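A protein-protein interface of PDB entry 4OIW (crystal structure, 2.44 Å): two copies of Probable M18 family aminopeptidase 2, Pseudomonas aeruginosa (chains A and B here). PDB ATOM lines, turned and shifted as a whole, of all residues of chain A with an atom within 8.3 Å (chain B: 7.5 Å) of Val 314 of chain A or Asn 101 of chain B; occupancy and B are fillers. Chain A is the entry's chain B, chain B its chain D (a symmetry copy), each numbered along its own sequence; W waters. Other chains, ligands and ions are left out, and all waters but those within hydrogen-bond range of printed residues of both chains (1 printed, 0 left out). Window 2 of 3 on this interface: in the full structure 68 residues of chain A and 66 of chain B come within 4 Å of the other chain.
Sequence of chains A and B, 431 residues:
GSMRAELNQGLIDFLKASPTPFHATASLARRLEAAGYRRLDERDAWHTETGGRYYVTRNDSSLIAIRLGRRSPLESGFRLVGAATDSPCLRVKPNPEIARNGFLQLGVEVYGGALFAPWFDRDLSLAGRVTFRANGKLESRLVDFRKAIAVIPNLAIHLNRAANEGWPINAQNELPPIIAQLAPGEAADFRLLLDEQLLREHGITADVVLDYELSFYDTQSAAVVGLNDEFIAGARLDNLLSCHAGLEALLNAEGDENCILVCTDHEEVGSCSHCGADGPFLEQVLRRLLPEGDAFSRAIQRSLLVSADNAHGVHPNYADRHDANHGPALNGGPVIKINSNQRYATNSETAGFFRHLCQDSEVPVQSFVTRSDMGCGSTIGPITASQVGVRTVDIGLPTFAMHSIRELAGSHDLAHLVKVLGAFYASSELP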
ATOM      1  N   ALA A 311     -23.212  22.957  30.144  1.00  0.00           N
ATOM      2  CA  ALA A 311     -22.886  24.252  29.543  1.00  0.00           C
ATOM      3  C   ALA A 311     -22.989  24.274  28.007  1.00  0.00           C
ATOM      4  O   ALA A 311     -23.089  23.228  27.323  1.00  0.00           O
ATOM      5  CB  ALA A 311     -21.469  24.656  29.953  1.00  0.00           C
ATOM      6  N   HIS A 312     -22.943  25.494  27.482  1.00  0.00           N
ATOM      7  CA  HIS A 312     -22.940  25.752  26.036  1.00  0.00           C
ATOM      8  C   HIS A 312     -21.554  25.892  25.429  1.00  0.00           C
ATOM      9  O   HIS A 312     -20.813  26.849  25.738  1.00  0.00           O
ATOM     10  CB  HIS A 312     -23.678  27.064  25.742  1.00  0.00           C
ATOM     11  CG  HIS A 312     -25.029  27.149  26.371  1.00  0.00           C
ATOM     12  ND1 HIS A 312     -26.110  26.437  25.902  1.00  0.00           N
ATOM     13  CD2 HIS A 312     -25.481  27.876  27.425  1.00  0.00           C
ATOM     14  CE1 HIS A 312     -27.172  26.730  26.635  1.00  0.00           C
ATOM     15  NE2 HIS A 312     -26.817  27.600  27.565  1.00  0.00           N
ATOM     16  N   GLY A 313     -21.238  24.983  24.505  1.00  0.00           N
ATOM     17  CA  GLY A 313     -20.057  25.149  23.647  1.00  0.00           C
ATOM     18  C   GLY A 313     -20.310  26.198  22.588  1.00  0.00           C
ATOM     19  O   GLY A 313     -21.439  26.422  22.201  1.00  0.00           O
ATOM     20  N   VAL A 314     -19.247  26.855  22.134  1.00  0.00           N
ATOM     21  CA  VAL A 314     -19.334  27.829  21.077  1.00  0.00           C
ATOM     22  C   VAL A 314     -19.600  27.103  19.775  1.00  0.00           C
ATOM     23  O   VAL A 314     -18.850  26.209  19.350  1.00  0.00           O
ATOM     24  CB  VAL A 314     -18.078  28.732  20.991  1.00  0.00           C
ATOM     25  CG1 VAL A 314     -16.779  27.962  20.740  1.00  0.00           C
ATOM     26  CG2 VAL A 314     -18.256  29.837  19.946  1.00  0.00           C
ATOM     27  N   HIS A 315     -20.698  27.489  19.152  1.00  0.00           N
ATOM     28  CA  HIS A 315     -21.219  26.771  18.012  1.00  0.00           C
ATOM     29  C   HIS A 315     -20.619  27.460  16.794  1.00  0.00           C
ATOM     30  O   HIS A 315     -20.797  28.659  16.654  1.00  0.00           O
ATOM     31  CB  HIS A 315     -22.765  26.858  18.064  1.00  0.00           C
ATOM     32  CG  HIS A 315     -23.471  26.043  17.027  1.00  0.00           C
ATOM     33  ND1 HIS A 315     -23.072  25.999  15.709  1.00  0.00           N
ATOM     34  CD2 HIS A 315     -24.569  25.262  17.105  1.00  0.00           C
ATOM     35  CE1 HIS A 315     -23.882  25.219  15.016  1.00  0.00           C
ATOM     36  NE2 HIS A 315     -24.794  24.750  15.839  1.00  0.00           N
ATOM     37  N   PRO A 316     -19.918  26.726  15.898  1.00  0.00           N
ATOM     38  CA  PRO A 316     -19.323  27.404  14.705  1.00  0.00           C
ATOM     39  C   PRO A 316     -20.293  28.122  13.704  1.00  0.00           C
ATOM     40  O   PRO A 316     -19.837  29.008  12.955  1.00  0.00           O
ATOM     41  CB  PRO A 316     -18.580  26.273  14.000  1.00  0.00           C
ATOM     42  CG  PRO A 316     -19.272  25.030  14.413  1.00  0.00           C
ATOM     43  CD  PRO A 316     -19.813  25.257  15.789  1.00  0.00           C
ATOM     44  N   ASN A 317     -21.579  27.748  13.666  1.00  0.00           N
ATOM     45  CA  ASN A 317     -22.549  28.468  12.824  1.00  0.00           C
ATOM     46  C   ASN A 317     -23.286  29.642  13.522  1.00  0.00           C
ATOM     47  O   ASN A 317     -24.114  30.305  12.919  1.00  0.00           O
ATOM     48  CB  ASN A 317     -23.598  27.491  12.233  1.00  0.00           C
ATOM     49  CG  ASN A 317     -22.983  26.436  11.343  1.00  0.00           C
ATOM     50  OD1 ASN A 317     -21.880  26.625  10.835  1.00  0.00           O
ATOM     51  ND2 ASN A 317     -23.692  25.289  11.161  1.00  0.00           N
ATOM     52  N   TYR A 318     -23.020  29.846  14.800  1.00  0.00           N
ATOM     53  CA  TYR A 318     -23.629  30.906  15.587  1.00  0.00           C
ATOM     54  C   TYR A 318     -22.613  31.384  16.666  1.00  0.00           C
ATOM     55  O   TYR A 318     -22.988  31.532  17.840  1.00  0.00           O
ATOM     56  CB  TYR A 318     -24.840  30.356  16.309  1.00  0.00           C
ATOM     57  CG  TYR A 318     -25.923  29.665  15.494  1.00  0.00           C
ATOM     58  CD1 TYR A 318     -26.965  30.384  14.946  1.00  0.00           C
ATOM     59  CD2 TYR A 318     -25.957  28.277  15.362  1.00  0.00           C
ATOM     60  CE1 TYR A 318     -27.958  29.757  14.203  1.00  0.00           C
ATOM     61  CE2 TYR A 318     -26.961  27.645  14.668  1.00  0.00           C
ATOM     62  CZ  TYR A 318     -27.967  28.393  14.064  1.00  0.00           C
ATOM     63  OH  TYR A 318     -29.020  27.778  13.366  1.00  0.00           O
ATOM     64  N   ALA A 319     -21.345  31.582  16.284  1.00  0.00           N
ATOM     65  CA  ALA A 319     -20.263  31.884  17.246  1.00  0.00           C
ATOM     66  C   ALA A 319     -20.465  33.186  18.033  1.00  0.00           C
ATOM     67  O   ALA A 319     -20.064  33.315  19.220  1.00  0.00           O
ATOM     68  CB  ALA A 319     -18.914  31.948  16.539  1.00  0.00           C
ATOM     69  N   ASP A 320     -21.068  34.162  17.384  1.00  0.00           N
ATOM     70  CA  ASP A 320     -21.278  35.472  18.042  1.00  0.00           C
ATOM     71  C   ASP A 320     -22.267  35.473  19.243  1.00  0.00           C
ATOM     72  O   ASP A 320     -22.372  36.477  19.922  1.00  0.00           O
ATOM     73  CB  ASP A 320     -21.661  36.543  17.003  1.00  0.00           C
ATOM     74  CG  ASP A 320     -22.959  36.221  16.262  1.00  0.00           C
ATOM     75  OD1 ASP A 320     -23.649  35.230  16.637  1.00  0.00           O
ATOM     76  OD2 ASP A 320     -23.288  36.954  15.281  1.00  0.00           O
ATOM     77  N   ARG A 321     -22.999  34.386  19.490  1.00  0.00           N
ATOM     78  CA  ARG A 321     -23.749  34.196  20.750  1.00  0.00           C
ATOM     79  C   ARG A 321     -22.890  33.964  22.017  1.00  0.00           C
ATOM     80  O   ARG A 321     -23.429  34.000  23.126  1.00  0.00           O
ATOM     81  CB  ARG A 321     -24.693  33.021  20.619  1.00  0.00           C
ATOM     82  CG  ARG A 321     -25.642  33.115  19.442  1.00  0.00           C
ATOM     83  CD  ARG A 321     -26.356  34.458  19.250  1.00  0.00           C
ATOM     84  NE  ARG A 321     -26.898  34.514  17.876  1.00  0.00           N
ATOM     85  CZ  ARG A 321     -28.193  34.430  17.533  1.00  0.00           C
ATOM     86  NH1 ARG A 321     -29.156  34.323  18.463  1.00  0.00           N
ATOM     87  NH2 ARG A 321     -28.535  34.454  16.239  1.00  0.00           N
ATOM     88  N   HIS A 322     -21.582  33.704  21.841  1.00  0.00           N
ATOM     89  CA  HIS A 322     -20.644  33.590  22.935  1.00  0.00           C
ATOM     90  C   HIS A 322     -19.745  34.768  22.973  1.00  0.00           C
ATOM     91  O   HIS A 322     -19.555  35.436  21.976  1.00  0.00           O
ATOM     92  CB  HIS A 322     -19.741  32.366  22.810  1.00  0.00           C
ATOM     93  CG  HIS A 322     -20.384  31.137  23.302  1.00  0.00           C
ATOM     94  ND1 HIS A 322     -21.379  30.496  22.601  1.00  0.00           N
ATOM     95  CD2 HIS A 322     -20.231  30.459  24.460  1.00  0.00           C
ATOM     96  CE1 HIS A 322     -21.772  29.438  23.283  1.00  0.00           C
ATOM     97  NE2 HIS A 322     -21.091  29.397  24.418  1.00  0.00           N
ATOM     98  N   ASP A 323     -19.209  34.994  24.172  1.00  0.00           N
ATOM     99  CA  ASP A 323     -18.094  35.881  24.411  1.00  0.00           C
ATOM    100  C   ASP A 323     -16.862  35.292  23.697  1.00  0.00           C
ATOM    101  O   ASP A 323     -16.541  34.115  23.855  1.00  0.00           O
ATOM    102  CB  ASP A 323     -17.868  35.985  25.925  1.00  0.00           C
ATOM    103  CG  ASP A 323     -16.709  36.873  26.275  1.00  0.00           C
ATOM    104  OD1 ASP A 323     -15.571  36.490  25.940  1.00  0.00           O
ATOM    105  OD2 ASP A 323     -16.942  37.949  26.884  1.00  0.00           O
ATOM    106  N   ALA A 324     -16.199  36.117  22.897  1.00  0.00           N
ATOM    107  CA  ALA A 324     -15.016  35.674  22.116  1.00  0.00           C
ATOM    108  C   ALA A 324     -13.985  34.916  23.027  1.00  0.00           C
ATOM    109  O   ALA A 324     -13.367  33.935  22.624  1.00  0.00           O
ATOM    110  CB  ALA A 324     -14.378  36.874  21.379  1.00  0.00           C
ATOM    111  N   ASN A 325     -13.873  35.328  24.277  1.00  0.00           N
ATOM    112  CA  ASN A 325     -12.899  34.713  25.198  1.00  0.00           C
ATOM    113  C   ASN A 325     -13.412  33.534  26.019  1.00  0.00           C
ATOM    114  O   ASN A 325     -12.636  32.897  26.697  1.00  0.00           O
ATOM    115  CB  ASN A 325     -12.344  35.777  26.176  1.00  0.00           C
ATOM    116  CG  ASN A 325     -11.337  36.706  25.529  1.00  0.00           C
ATOM    117  OD1 ASN A 325     -10.941  36.513  24.395  1.00  0.00           O
ATOM    118  ND2 ASN A 325     -10.909  37.716  26.266  1.00  0.00           N
ATOM    119  N   HIS A 326     -14.710  33.265  26.021  1.00  0.00           N
ATOM    120  CA  HIS A 326     -15.251  32.223  26.892  1.00  0.00           C
ATOM    121  C   HIS A 326     -16.163  31.325  26.072  1.00  0.00           C
ATOM    122  O   HIS A 326     -17.373  31.225  26.342  1.00  0.00           O
ATOM    123  CB  HIS A 326     -16.007  32.819  28.057  1.00  0.00           C
ATOM    124  CG  HIS A 326     -15.210  33.789  28.882  1.00  0.00           C
ATOM    125  ND1 HIS A 326     -15.061  35.118  28.536  1.00  0.00           N
ATOM    126  CD2 HIS A 326     -14.546  33.629  30.049  1.00  0.00           C
ATOM    127  CE1 HIS A 326     -14.336  35.727  29.452  1.00  0.00           C
ATOM    128  NE2 HIS A 326     -14.011  34.846  30.377  1.00  0.00           N
ATOM    129  N   GLY A 327     -15.552  30.707  25.050  1.00  0.00           N
ATOM    130  CA  GLY A 327     -16.194  29.728  24.200  1.00  0.00           C
ATOM    131  C   GLY A 327     -15.689  28.338  24.512  1.00  0.00           C
ATOM    132  O   GLY A 327     -14.617  27.972  24.061  1.00  0.00           O
ATOM    133  N   PRO A 328     -16.442  27.563  25.307  1.00  0.00           N
ATOM    134  CA  PRO A 328     -15.943  26.222  25.595  1.00  0.00           C
ATOM    135  C   PRO A 328     -15.942  25.317  24.371  1.00  0.00           C
ATOM    136  O   PRO A 328     -16.812  25.437  23.509  1.00  0.00           O
ATOM    137  CB  PRO A 328     -16.940  25.682  26.636  1.00  0.00           C
ATOM    138  CG  PRO A 328     -17.640  26.877  27.202  1.00  0.00           C
ATOM    139  CD  PRO A 328     -17.632  27.898  26.107  1.00  0.00           C
ATOM    140  N   ALA A 329     -14.958  24.424  24.292  1.00  0.00           N
ATOM    141  CA  ALA A 329     -14.899  23.475  23.197  1.00  0.00           C
ATOM    142  C   ALA A 329     -15.474  22.141  23.643  1.00  0.00           C
ATOM    143  O   ALA A 329     -15.232  21.710  24.777  1.00  0.00           O
ATOM    144  CB  ALA A 329     -13.462  23.298  22.712  1.00  0.00           C
ATOM    145  N   LEU A 330     -16.254  21.506  22.770  1.00  0.00           N
ATOM    146  CA  LEU A 330     -16.629  20.130  23.003  1.00  0.00           C
ATOM    147  C   LEU A 330     -15.325  19.335  23.065  1.00  0.00           C
ATOM    148  O   LEU A 330     -14.394  19.612  22.284  1.00  0.00           O
ATOM    149  CB  LEU A 330     -17.543  19.597  21.905  1.00  0.00           C
ATOM    150  CG  LEU A 330     -19.033  19.680  22.233  1.00  0.00           C
ATOM    151  CD1 LEU A 330     -19.413  21.121  22.483  1.00  0.00           C
ATOM    152  CD2 LEU A 330     -19.930  19.093  21.146  1.00  0.00           C
ATOM    153  N   GLN A 366     -12.303  24.438  31.639  1.00  0.00           N
ATOM    154  CA  GLN A 366     -12.682  25.580  30.830  1.00  0.00           C
ATOM    155  C   GLN A 366     -13.536  26.519  31.680  1.00  0.00           C
ATOM    156  O   GLN A 366     -14.111  26.098  32.682  1.00  0.00           O
ATOM    157  CB  GLN A 366     -13.480  25.100  29.623  1.00  0.00           C
ATOM    158  CG  GLN A 366     -12.762  24.065  28.773  1.00  0.00           C
ATOM    159  CD  GLN A 366     -13.540  23.682  27.542  1.00  0.00           C
ATOM    160  OE1 GLN A 366     -14.383  22.750  27.520  1.00  0.00           O
ATOM    161  NE2 GLN A 366     -13.259  24.373  26.506  1.00  0.00           N
ATOM    162  N   PHE A 368     -16.709  29.661  31.501  1.00  0.00           N
ATOM    163  CA  PHE A 368     -17.787  30.310  30.725  1.00  0.00           C
ATOM    164  C   PHE A 368     -18.391  31.408  31.577  1.00  0.00           C
ATOM    165  O   PHE A 368     -18.601  31.225  32.807  1.00  0.00           O
ATOM    166  CB  PHE A 368     -18.853  29.260  30.320  1.00  0.00           C
ATOM    167  CG  PHE A 368     -20.172  29.837  29.852  1.00  0.00           C
ATOM    168  CD1 PHE A 368     -21.186  30.155  30.761  1.00  0.00           C
ATOM    169  CD2 PHE A 368     -20.418  30.048  28.493  1.00  0.00           C
ATOM    170  CE1 PHE A 368     -22.404  30.713  30.328  1.00  0.00           C
ATOM    171  CE2 PHE A 368     -21.639  30.586  28.060  1.00  0.00           C
ATOM    172  CZ  PHE A 368     -22.636  30.911  28.981  1.00  0.00           C
ATOM    173  N   PRO A 398     -19.724  20.825  28.081  1.00  0.00           N
ATOM    174  CA  PRO A 398     -20.163  21.598  26.940  1.00  0.00           C
ATOM    175  C   PRO A 398     -20.985  20.853  25.910  1.00  0.00           C
ATOM    176  O   PRO A 398     -20.617  19.754  25.504  1.00  0.00           O
ATOM    177  CB  PRO A 398     -18.853  22.037  26.291  1.00  0.00           C
ATOM    178  CG  PRO A 398     -17.823  21.073  26.754  1.00  0.00           C
ATOM    179  CD  PRO A 398     -18.279  20.564  28.067  1.00  0.00           C
ATOM    180  N   THR A 399     -22.060  21.481  25.468  1.00  0.00           N
ATOM    181  CA  THR A 399     -22.963  20.894  24.485  1.00  0.00           C
ATOM    182  C   THR A 399     -23.559  21.926  23.515  1.00  0.00           C
ATOM    183  O   THR A 399     -23.552  23.121  23.819  1.00  0.00           O
ATOM    184  CB  THR A 399     -24.198  20.260  25.181  1.00  0.00           C
ATOM    185  OG1 THR A 399     -24.930  21.296  25.834  1.00  0.00           O
ATOM    186  CG2 THR A 399     -23.787  19.273  26.194  1.00  0.00           C
ATOM    187  N   PHE A 400     -24.134  21.426  22.411  1.00  0.00           N
ATOM    188  CA  PHE A 400     -24.903  22.210  21.494  1.00  0.00           C
ATOM    189  C   PHE A 400     -26.362  21.866  21.593  1.00  0.00           C
ATOM    190  O   PHE A 400     -26.696  20.786  22.021  1.00  0.00           O
ATOM    191  CB  PHE A 400     -24.468  21.949  20.062  1.00  0.00           C
ATOM    192  CG  PHE A 400     -23.045  22.338  19.762  1.00  0.00           C
ATOM    193  CD1 PHE A 400     -22.480  23.469  20.308  1.00  0.00           C
ATOM    194  CD2 PHE A 400     -22.274  21.581  18.895  1.00  0.00           C
ATOM    195  CE1 PHE A 400     -21.168  23.839  20.006  1.00  0.00           C
ATOM    196  CE2 PHE A 400     -20.982  21.942  18.587  1.00  0.00           C
ATOM    197  CZ  PHE A 400     -20.427  23.090  19.144  1.00  0.00           C
ATOM    198  N   ALA B  99     -13.102  25.621   8.422  1.00  0.00           N
ATOM    199  CA  ALA B  99     -12.377  25.364   9.699  1.00  0.00           C
ATOM    200  C   ALA B  99     -12.586  26.498  10.703  1.00  0.00           C
ATOM    201  O   ALA B  99     -11.974  27.549  10.596  1.00  0.00           O
ATOM    202  CB  ALA B  99     -10.867  25.193   9.455  1.00  0.00           C
ATOM    203  N   ARG B 100     -13.395  26.267  11.718  1.00  0.00           N
ATOM    204  CA  ARG B 100     -13.683  27.299  12.685  1.00  0.00           C
ATOM    205  C   ARG B 100     -13.946  26.746  14.035  1.00  0.00           C
ATOM    206  O   ARG B 100     -14.561  25.687  14.169  1.00  0.00           O
ATOM    207  CB  ARG B 100     -14.946  28.019  12.278  1.00  0.00           C
ATOM    208  CG  ARG B 100     -14.764  28.998  11.164  1.00  0.00           C
ATOM    209  CD  ARG B 100     -15.982  29.856  11.064  1.00  0.00           C
ATOM    210  NE  ARG B 100     -17.143  28.969  11.044  1.00  0.00           N
ATOM    211  CZ  ARG B 100     -18.069  28.918  10.077  1.00  0.00           C
ATOM    212  NH1 ARG B 100     -18.035  29.754   9.012  1.00  0.00           N
ATOM    213  NH2 ARG B 100     -19.065  28.036  10.202  1.00  0.00           N
ATOM    214  N   ASN B 101     -13.531  27.502  15.043  1.00  0.00           N
ATOM    215  CA  ASN B 101     -13.669  27.068  16.437  1.00  0.00           C
ATOM    216  C   ASN B 101     -13.224  25.630  16.680  1.00  0.00           C
ATOM    217  O   ASN B 101     -13.778  24.940  17.506  1.00  0.00           O
ATOM    218  CB  ASN B 101     -15.134  27.239  16.834  1.00  0.00           C
ATOM    219  CG  ASN B 101     -15.616  28.651  16.617  1.00  0.00           C
ATOM    220  OD1 ASN B 101     -16.367  28.930  15.679  1.00  0.00           O
ATOM    221  ND2 ASN B 101     -15.138  29.575  17.470  1.00  0.00           N
ATOM    222  N   GLY B 102     -12.223  25.163  15.937  1.00  0.00           N
ATOM    223  CA  GLY B 102     -11.702  23.806  16.151  1.00  0.00           C
ATOM    224  C   GLY B 102     -12.475  22.726  15.425  1.00  0.00           C
ATOM    225  O   GLY B 102     -12.138  21.571  15.555  1.00  0.00           O
ATOM    226  N   PHE B 103     -13.466  23.087  14.620  1.00  0.00           N
ATOM    227  CA  PHE B 103     -14.194  22.111  13.850  1.00  0.00           C
ATOM    228  C   PHE B 103     -13.805  22.069  12.382  1.00  0.00           C
ATOM    229  O   PHE B 103     -13.213  22.979  11.818  1.00  0.00           O
ATOM    230  CB  PHE B 103     -15.696  22.383  13.902  1.00  0.00           C
ATOM    231  CG  PHE B 103     -16.266  22.376  15.281  1.00  0.00           C
ATOM    232  CD1 PHE B 103     -16.651  21.183  15.870  1.00  0.00           C
ATOM    233  CD2 PHE B 103     -16.402  23.564  16.004  1.00  0.00           C
ATOM    234  CE1 PHE B 103     -17.148  21.166  17.145  1.00  0.00           C
ATOM    235  CE2 PHE B 103     -16.907  23.563  17.273  1.00  0.00           C
ATOM    236  CZ  PHE B 103     -17.281  22.373  17.846  1.00  0.00           C
ATOM    237  N   LEU B 104     -14.174  20.971  11.767  1.00  0.00           N
ATOM    238  CA  LEU B 104     -14.208  20.866  10.347  1.00  0.00           C
ATOM    239  C   LEU B 104     -15.684  20.753   9.963  1.00  0.00           C
ATOM    240  O   LEU B 104     -16.398  19.924  10.500  1.00  0.00           O
ATOM    241  CB  LEU B 104     -13.482  19.609   9.890  1.00  0.00           C
ATOM    242  CG  LEU B 104     -13.512  19.388   8.378  1.00  0.00           C
ATOM    243  CD1 LEU B 104     -12.871  20.569   7.674  1.00  0.00           C
ATOM    244  CD2 LEU B 104     -12.776  18.120   8.052  1.00  0.00           C
ATOM    245  N   GLN B 105     -16.114  21.615   9.052  1.00  0.00           N
ATOM    246  CA  GLN B 105     -17.422  21.541   8.440  1.00  0.00           C
ATOM    247  C   GLN B 105     -17.314  21.495   6.940  1.00  0.00           C
ATOM    248  O   GLN B 105     -16.283  21.887   6.354  1.00  0.00           O
ATOM    249  CB  GLN B 105     -18.217  22.775   8.801  1.00  0.00           C
ATOM    250  CG  GLN B 105     -18.404  22.937  10.297  1.00  0.00           C
ATOM    251  CD  GLN B 105     -19.036  24.250  10.641  1.00  0.00           C
ATOM    252  OE1 GLN B 105     -18.335  25.228  10.959  1.00  0.00           O
ATOM    253  NE2 GLN B 105     -20.362  24.301  10.574  1.00  0.00           N
ATOM    254  N   LEU B 155     -28.816  25.805  17.538  1.00  0.00           N
ATOM    255  CA  LEU B 155     -28.427  26.639  18.661  1.00  0.00           C
ATOM    256  C   LEU B 155     -29.373  26.406  19.855  1.00  0.00           C
ATOM    257  O   LEU B 155     -30.560  26.283  19.693  1.00  0.00           O
ATOM    258  CB  LEU B 155     -28.521  28.095  18.242  1.00  0.00           C
ATOM    259  CG  LEU B 155     -28.084  29.152  19.259  1.00  0.00           C
ATOM    260  CD1 LEU B 155     -26.644  28.924  19.679  1.00  0.00           C
ATOM    261  CD2 LEU B 155     -28.267  30.544  18.648  1.00  0.00           C
ATOM    262  N   LEU B 159     -29.709  30.622  24.139  1.00  0.00           N
ATOM    263  CA  LEU B 159     -28.950  31.592  23.349  1.00  0.00           C
ATOM    264  C   LEU B 159     -29.743  32.091  22.148  1.00  0.00           C
ATOM    265  O   LEU B 159     -29.227  32.847  21.319  1.00  0.00           O
ATOM    266  CB  LEU B 159     -27.629  30.987  22.869  1.00  0.00           C
ATOM    267  CG  LEU B 159     -26.729  30.488  23.992  1.00  0.00           C
ATOM    268  CD1 LEU B 159     -25.566  29.713  23.405  1.00  0.00           C
ATOM    269  CD2 LEU B 159     -26.210  31.644  24.817  1.00  0.00           C
ATOM    270  N   ILE B 178     -21.152  19.876  10.719  1.00  0.00           N
ATOM    271  CA  ILE B 178     -19.918  19.530  11.409  1.00  0.00           C
ATOM    272  C   ILE B 178     -19.597  18.061  11.133  1.00  0.00           C
ATOM    273  O   ILE B 178     -20.493  17.225  11.209  1.00  0.00           O
ATOM    274  CB  ILE B 178     -20.106  19.733  12.919  1.00  0.00           C
ATOM    275  CG1 ILE B 178     -20.359  21.195  13.242  1.00  0.00           C
ATOM    276  CG2 ILE B 178     -18.841  19.355  13.671  1.00  0.00           C
ATOM    277  CD1 ILE B 178     -20.693  21.440  14.702  1.00  0.00           C
ATOM    278  N   GLN B 181     -13.498  17.254  14.576  1.00  0.00           N
ATOM    279  CA  GLN B 181     -12.649  18.338  15.118  1.00  0.00           C
ATOM    280  C   GLN B 181     -11.248  18.274  14.554  1.00  0.00           C
ATOM    281  O   GLN B 181     -10.787  17.215  14.208  1.00  0.00           O
ATOM    282  CB  GLN B 181     -12.581  18.278  16.623  1.00  0.00           C
ATOM    283  CG  GLN B 181     -13.886  18.758  17.192  1.00  0.00           C
ATOM    284  CD  GLN B 181     -14.024  18.548  18.679  1.00  0.00           C
ATOM    285  OE1 GLN B 181     -13.865  17.440  19.178  1.00  0.00           O
ATOM    286  NE2 GLN B 181     -14.375  19.612  19.386  1.00  0.00           N
ATOM    287  N   LEU B 182     -10.620  19.423  14.408  1.00  0.00           N
ATOM    288  CA  LEU B 182      -9.239  19.540  13.975  1.00  0.00           C
ATOM    289  C   LEU B 182      -8.349  20.110  15.052  1.00  0.00           C
ATOM    290  O   LEU B 182      -8.685  21.108  15.633  1.00  0.00           O
ATOM    291  CB  LEU B 182      -9.156  20.551  12.829  1.00  0.00           C
ATOM    292  CG  LEU B 182      -9.889  20.169  11.551  1.00  0.00           C
ATOM    293  CD1 LEU B 182      -9.701  21.282  10.558  1.00  0.00           C
ATOM    294  CD2 LEU B 182      -9.361  18.844  11.006  1.00  0.00           C
HETATM  295  O   HOH W   1     -30.780  26.652  15.498  1.00  0.00           O
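OD1 of Asn 317 of chain A lies within hydrogen-bond range of NE2 of Gln 105 of chain B, 2.8 Å away.
O of Leu 159 of chain B lies within hydrogen-bond range of NH1 of Arg 321 of chain A (3.2 Å).
OD1 of Asn 317 of chain A sits at hydrogen-bond distance from NH2 of Arg 100 of chain B, 3.2 Å away.
NH2 of Arg 100 of chain B lies within hydrogen-bond range of O of Pro 316 of chain A.
The backbone carbonyl oxygen (O) of Leu 330 of chain A is in hydrogen-bond range of the side-chain amide nitrogen (NE2) of Gln 181 of chain B.
A ring nitrogen (ND1) of His 315 of chain A sits at hydrogen-bond distance from the backbone NH (N) of Asn 317 of chain A, at 3.1 Å.
The backbone NH (N) of Val 314 of chain A sits at hydrogen-bond distance from the backbone carbonyl oxygen (O) of Pro 328 of chain A (3.1 Å).
O of His 312 of chain A is in hydrogen-bond range of NE2 of His 322 of chain A, at 2.9 Å.
The side-chain carboxylate of Asp 320 of chain A is in salt-bridge range of the guanidinium group of Arg 321 of chain A.
The side-chain amide oxygen (OE1) of Gln 105 of chain B sits at hydrogen-bond distance from the guanidinium group (NH2) of Arg 100 of chain B, 3.0 Å away.
Among the printed residues, pairs that only touch across the chains: His 312 of chain A with Leu 159 of chain B (3.96 Å), Val 314 of chain A with Asn 101 of chain B (3.99 Å), Val 314 of chain A with Phe 103 of chain B (3.9 Å), Pro 316 of chain A with Asn 101 of chain B (3.5 Å), Pro 316 of chain A with Phe 103 of chain B (3.6 Å), Pro 316 of chain A with Gln 105 of chain B (3.2 Å), Pro 316 of chain A with Ile 178 of chain B (3.9 Å), Tyr 318 of chain A with Leu 155 of chain B (3.9 Å), Arg 321 of chain A with Leu 155 of chain B (3.8 Å), His 322 of chain A with Leu 159 of chain B (3.8 Å), Phe 400 of chain A with Phe 103 of chain B (3.5 Å) and Phe 400 of chain A with Ile 178 of chain B (3.9 Å).
Of the printed residues of chain B, Val 314 of chain A touches Asn 101 (3.99 Å) and Phe 103 (3.9 Å).
Pro 328 of chain A touches none of the printed residues of chain B.
Printed residues of chain A within 4 Å of Arg 100 of chain B: Pro 316 and Asn 317.
Of the printed residues of chain A, Asn 101 of chain B touches Val 314 (3.99 Å) and Pro 316 (3.5 Å).
No residue of chain A comes within 4 Å of Gly 102 of chain B.
Of the printed residues of chain A, Leu 155 of chain B touches Tyr 318 and Arg 321.
Leu 182 of chain B touches none of the printed residues of chain A.
The nearest printed residue of chain A that does not touch Asn 101 of chain B is Ala 319 of chain A (4.04 Å).
The nearest printed residue of chain B that does not touch Tyr 318 of chain A is Arg 100 of chain B (6.3 Å).
Of the 25 printed residues of chain A, 9 touch a printed residue of chain B.
Among the printed residues, no Asp or Glu carboxylate lies within 4 Å of a Lys or Arg side-chain nitrogen of the other chain.
No position is printed for both chains.
Of the 17 pairs that touch across the chains among the printed residues, none has its exchanged pair printed and touching as well.
Water W1 lies within hydrogen-bond range of N of Leu 155 of chain B (3.0 Å) and OH of Tyr 318 of chain A (3.0 Å).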
